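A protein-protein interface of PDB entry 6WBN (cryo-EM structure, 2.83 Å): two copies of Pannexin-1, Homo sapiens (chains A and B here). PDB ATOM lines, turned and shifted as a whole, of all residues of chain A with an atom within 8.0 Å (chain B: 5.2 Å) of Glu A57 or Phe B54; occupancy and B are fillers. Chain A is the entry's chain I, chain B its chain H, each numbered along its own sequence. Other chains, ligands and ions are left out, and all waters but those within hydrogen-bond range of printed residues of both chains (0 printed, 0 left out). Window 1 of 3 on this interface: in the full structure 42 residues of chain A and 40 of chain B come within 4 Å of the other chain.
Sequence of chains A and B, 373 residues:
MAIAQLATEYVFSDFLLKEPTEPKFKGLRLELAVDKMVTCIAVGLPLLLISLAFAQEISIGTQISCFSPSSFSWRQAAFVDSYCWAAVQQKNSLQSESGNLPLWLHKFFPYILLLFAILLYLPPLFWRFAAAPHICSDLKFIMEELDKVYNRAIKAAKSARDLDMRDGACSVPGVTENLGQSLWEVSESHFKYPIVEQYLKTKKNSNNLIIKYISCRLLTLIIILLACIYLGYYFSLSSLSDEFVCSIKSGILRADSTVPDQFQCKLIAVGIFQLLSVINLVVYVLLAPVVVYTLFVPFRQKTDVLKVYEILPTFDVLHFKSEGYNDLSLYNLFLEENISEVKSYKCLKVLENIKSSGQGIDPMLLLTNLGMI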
ATOM      1  N   ALA A   2       6.567  21.158   8.441  1.00  0.00           N
ATOM      2  CA  ALA A   2       6.095  20.151   7.504  1.00  0.00           C
ATOM      3  C   ALA A   2       4.581  20.113   7.497  1.00  0.00           C
ATOM      4  O   ALA A   2       3.946  20.374   8.508  1.00  0.00           O
ATOM      5  CB  ALA A   2       6.659  18.791   7.858  1.00  0.00           C
ATOM      6  N   ILE A   3       4.013  19.777   6.335  1.00  0.00           N
ATOM      7  CA  ILE A   3       2.530  19.724   6.155  1.00  0.00           C
ATOM      8  C   ILE A   3       1.936  18.616   7.033  1.00  0.00           C
ATOM      9  O   ILE A   3       0.812  18.809   7.531  1.00  0.00           O
ATOM     10  CB  ILE A   3       2.165  19.534   4.670  1.00  0.00           C
ATOM     11  CG1 ILE A   3       2.274  20.846   3.888  1.00  0.00           C
ATOM     12  CG2 ILE A   3       0.787  18.908   4.530  1.00  0.00           C
ATOM     13  CD1 ILE A   3       2.004  20.700   2.408  1.00  0.00           C
ATOM     14  N   ALA A   4       2.660  17.506   7.214  1.00  0.00           N
ATOM     15  CA  ALA A   4       2.144  16.406   8.011  1.00  0.00           C
ATOM     16  C   ALA A   4       2.163  16.721   9.499  1.00  0.00           C
ATOM     17  O   ALA A   4       1.288  16.257  10.237  1.00  0.00           O
ATOM     18  CB  ALA A   4       2.946  15.144   7.728  1.00  0.00           C
ATOM     19  N   GLN A   5       3.137  17.500   9.960  1.00  0.00           N
ATOM     20  CA  GLN A   5       3.159  17.877  11.367  1.00  0.00           C
ATOM     21  C   GLN A   5       1.969  18.755  11.711  1.00  0.00           C
ATOM     22  O   GLN A   5       1.336  18.579  12.757  1.00  0.00           O
ATOM     23  CB  GLN A   5       4.467  18.578  11.705  1.00  0.00           C
ATOM     24  CG  GLN A   5       5.662  17.664  11.648  1.00  0.00           C
ATOM     25  CD  GLN A   5       6.923  18.339  12.129  1.00  0.00           C
ATOM     26  OE1 GLN A   5       6.872  19.285  12.914  1.00  0.00           O
ATOM     27  NE2 GLN A   5       8.070  17.854  11.665  1.00  0.00           N
ATOM     28  N   LEU A   6       1.652  19.717  10.845  1.00  0.00           N
ATOM     29  CA  LEU A   6       0.456  20.517  11.063  1.00  0.00           C
ATOM     30  C   LEU A   6      -0.779  19.640  11.071  1.00  0.00           C
ATOM     31  O   LEU A   6      -1.679  19.831  11.895  1.00  0.00           O
ATOM     32  CB  LEU A   6       0.327  21.592   9.990  1.00  0.00           C
ATOM     33  CG  LEU A   6       1.598  22.368   9.703  1.00  0.00           C
ATOM     34  CD1 LEU A   6       1.416  23.193   8.456  1.00  0.00           C
ATOM     35  CD2 LEU A   6       1.943  23.238  10.883  1.00  0.00           C
ATOM     36  N   LEU A  52      -1.028  26.330   6.920  1.00  0.00           N
ATOM     37  CA  LEU A  52      -0.829  25.772   5.590  1.00  0.00           C
ATOM     38  C   LEU A  52      -0.397  26.835   4.599  1.00  0.00           C
ATOM     39  O   LEU A  52       0.437  26.573   3.730  1.00  0.00           O
ATOM     40  CB  LEU A  52      -2.103  25.090   5.117  1.00  0.00           C
ATOM     41  CG  LEU A  52      -2.150  23.575   5.217  1.00  0.00           C
ATOM     42  CD1 LEU A  52      -1.913  23.126   6.621  1.00  0.00           C
ATOM     43  CD2 LEU A  52      -3.503  23.130   4.762  1.00  0.00           C
ATOM     44  N   ALA A  53      -0.946  28.043   4.712  1.00  0.00           N
ATOM     45  CA  ALA A  53      -0.647  29.079   3.732  1.00  0.00           C
ATOM     46  C   ALA A  53       0.825  29.435   3.689  1.00  0.00           C
ATOM     47  O   ALA A  53       1.281  30.011   2.698  1.00  0.00           O
ATOM     48  CB  ALA A  53      -1.461  30.331   4.030  1.00  0.00           C
ATOM     49  N   PHE A  54       1.582  29.103   4.728  1.00  0.00           N
ATOM     50  CA  PHE A  54       3.010  29.386   4.769  1.00  0.00           C
ATOM     51  C   PHE A  54       3.823  28.122   4.979  1.00  0.00           C
ATOM     52  O   PHE A  54       4.948  28.193   5.472  1.00  0.00           O
ATOM     53  CB  PHE A  54       3.329  30.405   5.856  1.00  0.00           C
ATOM     54  CG  PHE A  54       2.604  31.690   5.690  1.00  0.00           C
ATOM     55  CD1 PHE A  54       3.021  32.610   4.759  1.00  0.00           C
ATOM     56  CD2 PHE A  54       1.489  31.969   6.442  1.00  0.00           C
ATOM     57  CE1 PHE A  54       2.349  33.783   4.592  1.00  0.00           C
ATOM     58  CE2 PHE A  54       0.816  33.144   6.274  1.00  0.00           C
ATOM     59  CZ  PHE A  54       1.246  34.052   5.348  1.00  0.00           C
ATOM     60  N   ALA A  55       3.263  26.967   4.639  1.00  0.00           N
ATOM     61  CA  ALA A  55       4.027  25.734   4.667  1.00  0.00           C
ATOM     62  C   ALA A  55       5.239  25.861   3.763  1.00  0.00           C
ATOM     63  O   ALA A  55       5.179  26.489   2.706  1.00  0.00           O
ATOM     64  CB  ALA A  55       3.158  24.561   4.226  1.00  0.00           C
ATOM     65  N   GLN A  56       6.347  25.266   4.186  1.00  0.00           N
ATOM     66  CA  GLN A  56       7.595  25.476   3.470  1.00  0.00           C
ATOM     67  C   GLN A  56       7.555  24.905   2.062  1.00  0.00           C
ATOM     68  O   GLN A  56       8.380  25.284   1.228  1.00  0.00           O
ATOM     69  CB  GLN A  56       8.751  24.863   4.246  1.00  0.00           C
ATOM     70  CG  GLN A  56      10.098  25.145   3.624  1.00  0.00           C
ATOM     71  CD  GLN A  56      10.430  26.625   3.626  1.00  0.00           C
ATOM     72  OE1 GLN A  56      10.504  27.253   4.683  1.00  0.00           O
ATOM     73  NE2 GLN A  56      10.616  27.193   2.440  1.00  0.00           N
ATOM     74  N   GLU A  57       6.617  24.010   1.775  1.00  0.00           N
ATOM     75  CA  GLU A  57       6.514  23.403   0.460  1.00  0.00           C
ATOM     76  C   GLU A  57       5.519  24.092  -0.454  1.00  0.00           C
ATOM     77  O   GLU A  57       5.447  23.745  -1.634  1.00  0.00           O
ATOM     78  CB  GLU A  57       6.170  21.922   0.596  1.00  0.00           C
ATOM     79  CG  GLU A  57       5.070  21.603   1.568  1.00  0.00           C
ATOM     80  CD  GLU A  57       5.643  21.259   2.926  1.00  0.00           C
ATOM     81  OE1 GLU A  57       6.761  21.721   3.223  1.00  0.00           O
ATOM     82  OE2 GLU A  57       5.010  20.507   3.687  1.00  0.00           O
ATOM     83  N   ILE A  58       4.749  25.041   0.051  1.00  0.00           N
ATOM     84  CA  ILE A  58       4.000  25.918  -0.834  1.00  0.00           C
ATOM     85  C   ILE A  58       4.665  27.280  -0.970  1.00  0.00           C
ATOM     86  O   ILE A  58       4.609  27.889  -2.041  1.00  0.00           O
ATOM     87  CB  ILE A  58       2.554  26.039  -0.342  1.00  0.00           C
ATOM     88  CG1 ILE A  58       1.834  24.725  -0.581  1.00  0.00           C
ATOM     89  CG2 ILE A  58       1.833  27.104  -1.081  1.00  0.00           C
ATOM     90  CD1 ILE A  58       1.664  24.422  -2.035  1.00  0.00           C
ATOM     91  N   SER A  59       5.329  27.760   0.073  1.00  0.00           N
ATOM     92  CA  SER A  59       5.941  29.077   0.033  1.00  0.00           C
ATOM     93  C   SER A  59       7.164  29.062  -0.868  1.00  0.00           C
ATOM     94  O   SER A  59       8.061  28.234  -0.703  1.00  0.00           O
ATOM     95  CB  SER A  59       6.336  29.532   1.433  1.00  0.00           C
ATOM     96  OG  SER A  59       5.297  29.284   2.355  1.00  0.00           O
ATOM     97  N   ILE A  60       7.195  29.988  -1.821  1.00  0.00           N
ATOM     98  CA  ILE A  60       8.331  30.080  -2.721  1.00  0.00           C
ATOM     99  C   ILE A  60       9.465  30.847  -2.074  1.00  0.00           C
ATOM    100  O   ILE A  60      10.632  30.650  -2.422  1.00  0.00           O
ATOM    101  CB  ILE A  60       7.908  30.740  -4.040  1.00  0.00           C
ATOM    102  CG1 ILE A  60       8.988  30.553  -5.088  1.00  0.00           C
ATOM    103  CG2 ILE A  60       7.651  32.208  -3.836  1.00  0.00           C
ATOM    104  CD1 ILE A  60       9.393  29.137  -5.226  1.00  0.00           C
ATOM    105  N   ILE A 272      -2.904  31.487  -2.963  1.00  0.00           N
ATOM    106  CA  ILE A 272      -3.049  30.537  -1.870  1.00  0.00           C
ATOM    107  C   ILE A 272      -4.040  31.056  -0.848  1.00  0.00           C
ATOM    108  O   ILE A 272      -4.872  30.303  -0.331  1.00  0.00           O
ATOM    109  CB  ILE A 272      -1.680  30.263  -1.238  1.00  0.00           C
ATOM    110  CG1 ILE A 272      -0.708  29.809  -2.311  1.00  0.00           C
ATOM    111  CG2 ILE A 272      -1.792  29.228  -0.174  1.00  0.00           C
ATOM    112  CD1 ILE A 272       0.692  30.232  -2.047  1.00  0.00           C
ATOM    113  N   ILE B  50       3.612  12.720   1.792  1.00  0.00           N
ATOM    114  CA  ILE B  50       3.842  14.159   1.760  1.00  0.00           C
ATOM    115  C   ILE B  50       5.178  14.490   2.397  1.00  0.00           C
ATOM    116  O   ILE B  50       5.954  15.294   1.873  1.00  0.00           O
ATOM    117  CB  ILE B  50       2.703  14.903   2.471  1.00  0.00           C
ATOM    118  CG1 ILE B  50       1.430  14.857   1.651  1.00  0.00           C
ATOM    119  CG2 ILE B  50       3.084  16.335   2.704  1.00  0.00           C
ATOM    120  CD1 ILE B  50       0.252  15.344   2.427  1.00  0.00           C
ATOM    121  N   SER B  51       5.464  13.886   3.548  1.00  0.00           N
ATOM    122  CA  SER B  51       6.729  14.170   4.208  1.00  0.00           C
ATOM    123  C   SER B  51       7.909  13.697   3.384  1.00  0.00           C
ATOM    124  O   SER B  51       8.963  14.335   3.394  1.00  0.00           O
ATOM    125  CB  SER B  51       6.757  13.530   5.585  1.00  0.00           C
ATOM    126  OG  SER B  51       5.620  13.912   6.328  1.00  0.00           O
ATOM    127  N   LEU B  52       7.757  12.591   2.663  1.00  0.00           N
ATOM    128  CA  LEU B  52       8.858  12.095   1.851  1.00  0.00           C
ATOM    129  C   LEU B  52       9.099  12.975   0.640  1.00  0.00           C
ATOM    130  O   LEU B  52      10.248  13.200   0.252  1.00  0.00           O
ATOM    131  CB  LEU B  52       8.581  10.662   1.418  1.00  0.00           C
ATOM    132  CG  LEU B  52       9.291   9.563   2.190  1.00  0.00           C
ATOM    133  CD1 LEU B  52       8.979   9.646   3.647  1.00  0.00           C
ATOM    134  CD2 LEU B  52       8.826   8.252   1.643  1.00  0.00           C
ATOM    135  N   ALA B  53       8.034  13.489   0.029  1.00  0.00           N
ATOM    136  CA  ALA B  53       8.191  14.263  -1.194  1.00  0.00           C
ATOM    137  C   ALA B  53       9.036  15.505  -0.996  1.00  0.00           C
ATOM    138  O   ALA B  53       9.548  16.053  -1.975  1.00  0.00           O
ATOM    139  CB  ALA B  53       6.827  14.662  -1.741  1.00  0.00           C
ATOM    140  N   PHE B  54       9.204  15.961   0.240  1.00  0.00           N
ATOM    141  CA  PHE B  54      10.015  17.134   0.531  1.00  0.00           C
ATOM    142  C   PHE B  54      11.128  16.814   1.512  1.00  0.00           C
ATOM    143  O   PHE B  54      11.611  17.710   2.201  1.00  0.00           O
ATOM    144  CB  PHE B  54       9.150  18.269   1.067  1.00  0.00           C
ATOM    145  CG  PHE B  54       8.063  18.671   0.138  1.00  0.00           C
ATOM    146  CD1 PHE B  54       8.338  19.449  -0.960  1.00  0.00           C
ATOM    147  CD2 PHE B  54       6.773  18.249   0.341  1.00  0.00           C
ATOM    148  CE1 PHE B  54       7.349  19.808  -1.825  1.00  0.00           C
ATOM    149  CE2 PHE B  54       5.781  18.607  -0.524  1.00  0.00           C
ATOM    150  CZ  PHE B  54       6.070  19.387  -1.608  1.00  0.00           C
ATOM    151  N   ALA B  55      11.519  15.549   1.606  1.00  0.00           N
ATOM    152  CA  ALA B  55      12.674  15.186   2.406  1.00  0.00           C
ATOM    153  C   ALA B  55      13.896  15.938   1.912  1.00  0.00           C
ATOM    154  O   ALA B  55      14.061  16.163   0.713  1.00  0.00           O
ATOM    155  CB  ALA B  55      12.915  13.682   2.337  1.00  0.00           C
ATOM    156  N   GLN B  56      14.754  16.334   2.844  1.00  0.00           N
ATOM    157  CA  GLN B  56      15.862  17.203   2.480  1.00  0.00           C
ATOM    158  C   GLN B  56      16.845  16.522   1.544  1.00  0.00           C
ATOM    159  O   GLN B  56      17.634  17.205   0.887  1.00  0.00           O
ATOM    160  CB  GLN B  56      16.583  17.680   3.733  1.00  0.00           C
ATOM    161  CG  GLN B  56      17.673  18.684   3.443  1.00  0.00           C
ATOM    162  CD  GLN B  56      17.125  19.969   2.851  1.00  0.00           C
ATOM    163  OE1 GLN B  56      16.313  20.653   3.475  1.00  0.00           O
ATOM    164  NE2 GLN B  56      17.555  20.294   1.638  1.00  0.00           N
ATOM    165  N   SER B  59      14.830  16.718  -2.058  1.00  0.00           N
ATOM    166  CA  SER B  59      14.581  18.069  -2.532  1.00  0.00           C
ATOM    167  C   SER B  59      15.883  18.726  -2.955  1.00  0.00           C
ATOM    168  O   SER B  59      16.848  18.767  -2.191  1.00  0.00           O
ATOM    169  CB  SER B  59      13.906  18.905  -1.452  1.00  0.00           C
ATOM    170  OG  SER B  59      12.857  18.185  -0.840  1.00  0.00           O
ATOM    171  N   GLN B  63      10.770  24.799  -5.480  1.00  0.00           N
ATOM    172  CA  GLN B  63       9.838  23.996  -6.255  1.00  0.00           C
ATOM    173  C   GLN B  63       9.723  24.432  -7.702  1.00  0.00           C
ATOM    174  O   GLN B  63       9.164  23.688  -8.508  1.00  0.00           O
ATOM    175  CB  GLN B  63       8.443  24.036  -5.638  1.00  0.00           C
ATOM    176  CG  GLN B  63       8.396  23.758  -4.170  1.00  0.00           C
ATOM    177  CD  GLN B  63       8.500  25.015  -3.359  1.00  0.00           C
ATOM    178  OE1 GLN B  63       8.390  26.114  -3.889  1.00  0.00           O
ATOM    179  NE2 GLN B  63       8.699  24.865  -2.061  1.00  0.00           N
ATOM    180  N   TRP B  85       5.482  31.340 -10.144  1.00  0.00           N
ATOM    181  CA  TRP B  85       4.900  30.501  -9.108  1.00  0.00           C
ATOM    182  C   TRP B  85       3.511  30.982  -8.734  1.00  0.00           C
ATOM    183  O   TRP B  85       2.571  30.191  -8.641  1.00  0.00           O
ATOM    184  CB  TRP B  85       5.805  30.491  -7.888  1.00  0.00           C
ATOM    185  CG  TRP B  85       5.326  29.648  -6.771  1.00  0.00           C
ATOM    186  CD1 TRP B  85       4.949  30.069  -5.542  1.00  0.00           C
ATOM    187  CD2 TRP B  85       5.192  28.229  -6.767  1.00  0.00           C
ATOM    188  NE1 TRP B  85       4.582  29.005  -4.768  1.00  0.00           N
ATOM    189  CE2 TRP B  85       4.725  27.861  -5.503  1.00  0.00           C
ATOM    190  CE3 TRP B  85       5.416  27.235  -7.712  1.00  0.00           C
ATOM    191  CZ2 TRP B  85       4.480  26.549  -5.161  1.00  0.00           C
ATOM    192  CZ3 TRP B  85       5.173  25.939  -7.370  1.00  0.00           C
ATOM    193  CH2 TRP B  85       4.710  25.604  -6.109  1.00  0.00           C
ATOM    194  N   PRO B 110       0.596  18.525  -2.367  1.00  0.00           N
ATOM    195  CA  PRO B 110       0.574  18.248  -0.926  1.00  0.00           C
ATOM    196  C   PRO B 110      -0.756  18.564  -0.283  1.00  0.00           C
ATOM    197  O   PRO B 110      -1.226  17.808   0.574  1.00  0.00           O
ATOM    198  CB  PRO B 110       1.682  19.151  -0.380  1.00  0.00           C
ATOM    199  CG  PRO B 110       2.520  19.457  -1.520  1.00  0.00           C
ATOM    200  CD  PRO B 110       1.639  19.507  -2.697  1.00  0.00           C
ATOM    201  N   PHE B 273       6.361  13.617  -7.212  1.00  0.00           N
ATOM    202  CA  PHE B 273       4.936  13.561  -6.922  1.00  0.00           C
ATOM    203  C   PHE B 273       4.276  12.412  -7.653  1.00  0.00           C
ATOM    204  O   PHE B 273       3.435  11.715  -7.088  1.00  0.00           O
ATOM    205  CB  PHE B 273       4.262  14.867  -7.311  1.00  0.00           C
ATOM    206  CG  PHE B 273       4.614  16.006  -6.433  1.00  0.00           C
ATOM    207  CD1 PHE B 273       5.297  15.801  -5.263  1.00  0.00           C
ATOM    208  CD2 PHE B 273       4.255  17.287  -6.775  1.00  0.00           C
ATOM    209  CE1 PHE B 273       5.621  16.850  -4.459  1.00  0.00           C
ATOM    210  CE2 PHE B 273       4.576  18.335  -5.970  1.00  0.00           C
ATOM    211  CZ  PHE B 273       5.259  18.118  -4.811  1.00  0.00           C
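Positions printed for both chains: 52, 53, 54, 55, 56 and 59.
Of the 10 pairs that touch across the chains among the printed residues, none has its exchanged pair printed and touching as well.
Of the 12 printed residues of chain B, 6 touch a printed residue of chain A.
Hydrophobic or aromatic side chains of chain B within 4 Å of the printed part of chain A: Ile B50, Phe B54, Trp B85 and Pro B110.
Of the 15 printed residues of chain A, 7 touch a printed residue of chain B.
Along chain A the printed residues that touch a printed residue of chain B span positions 3 to 60.
Among the printed residues, no Asp or Glu carboxylate lies within 4 Å of a Lys or Arg side-chain nitrogen of the other chain.
The side-chain carboxylate (OE2) of Glu A57 lies close to the backbone NH (N) of Ile A3 (2.9 Å).
The side-chain hydroxyl (OG) of Ser B59 sits close to the backbone carbonyl oxygen (O) of Phe B54 (3.3 Å).
O of Ala A55 is in hydrogen-bond range of OG of Ser A59 (2.8 Å).
The side-chain hydroxyl (OG) of Ser A59 lies close to the backbone carbonyl oxygen (O) of Phe A54 (3.3 Å).
Of the printed residues of chain B, Ala A4 touches Ser B51 (3.3 Å).
Glu A57 touches just these residues of chain B: Phe B54 (3.4 Å) and Gln B63 (3.5 Å).
Of the printed residues of chain B, Ile A60 touches Gln B63 (3.5 Å) and Trp B85 (3.4 Å).
Leu B52 touches none of the printed residues of chain A.
No residue of chain A comes within 4 Å of Ala B53.
Of chain A, only Glu A57 comes within 4 Å of Phe B54.
No residue of chain A comes within 4 Å of Ala B55.
Ser B59 touches none of the printed residues of chain A.
Of the printed residues of chain A, Trp B85 touches Ile A58 and Ile A60.
The nearest residue of chain B that does not touch Glu A57 is Pro B110 (4.5 Å).
The nearest residue of chain A that does not touch Phe B54 is Ile A3 (5.2 Å).
The nearest printed residue of chain B that does not touch Ser A59 is Trp B85 (4.7 Å).
The side-chain amide nitrogen (NE2) of Gln B63 sits at hydrogen-bond distance from the backbone carbonyl oxygen (O) of Gln A56, 3.3 Å away.
O of Ile A58 sits at hydrogen-bond distance from NE1 of Trp B85.
The side-chain amide nitrogen of Gln B63 sits at hydrogen-bond distance from the backbone carbonyl oxygen of Glu A57 (3.5 Å).
CG2 of Ile B50 touches CB of Ile A3, 3.9 Å away.
CD1 of Ile A3 touches CB of Pro B110 (3.2 Å).
Ala A4 touches Ser B51 (CB to OG, 3.3 Å).
Glu A57 touches Phe B54 (CB to CZ, 3.4 Å).
Gln B63 touches Ser A59.
Ile A60 touches Gln B63.
Ile A60 touches Trp B85.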
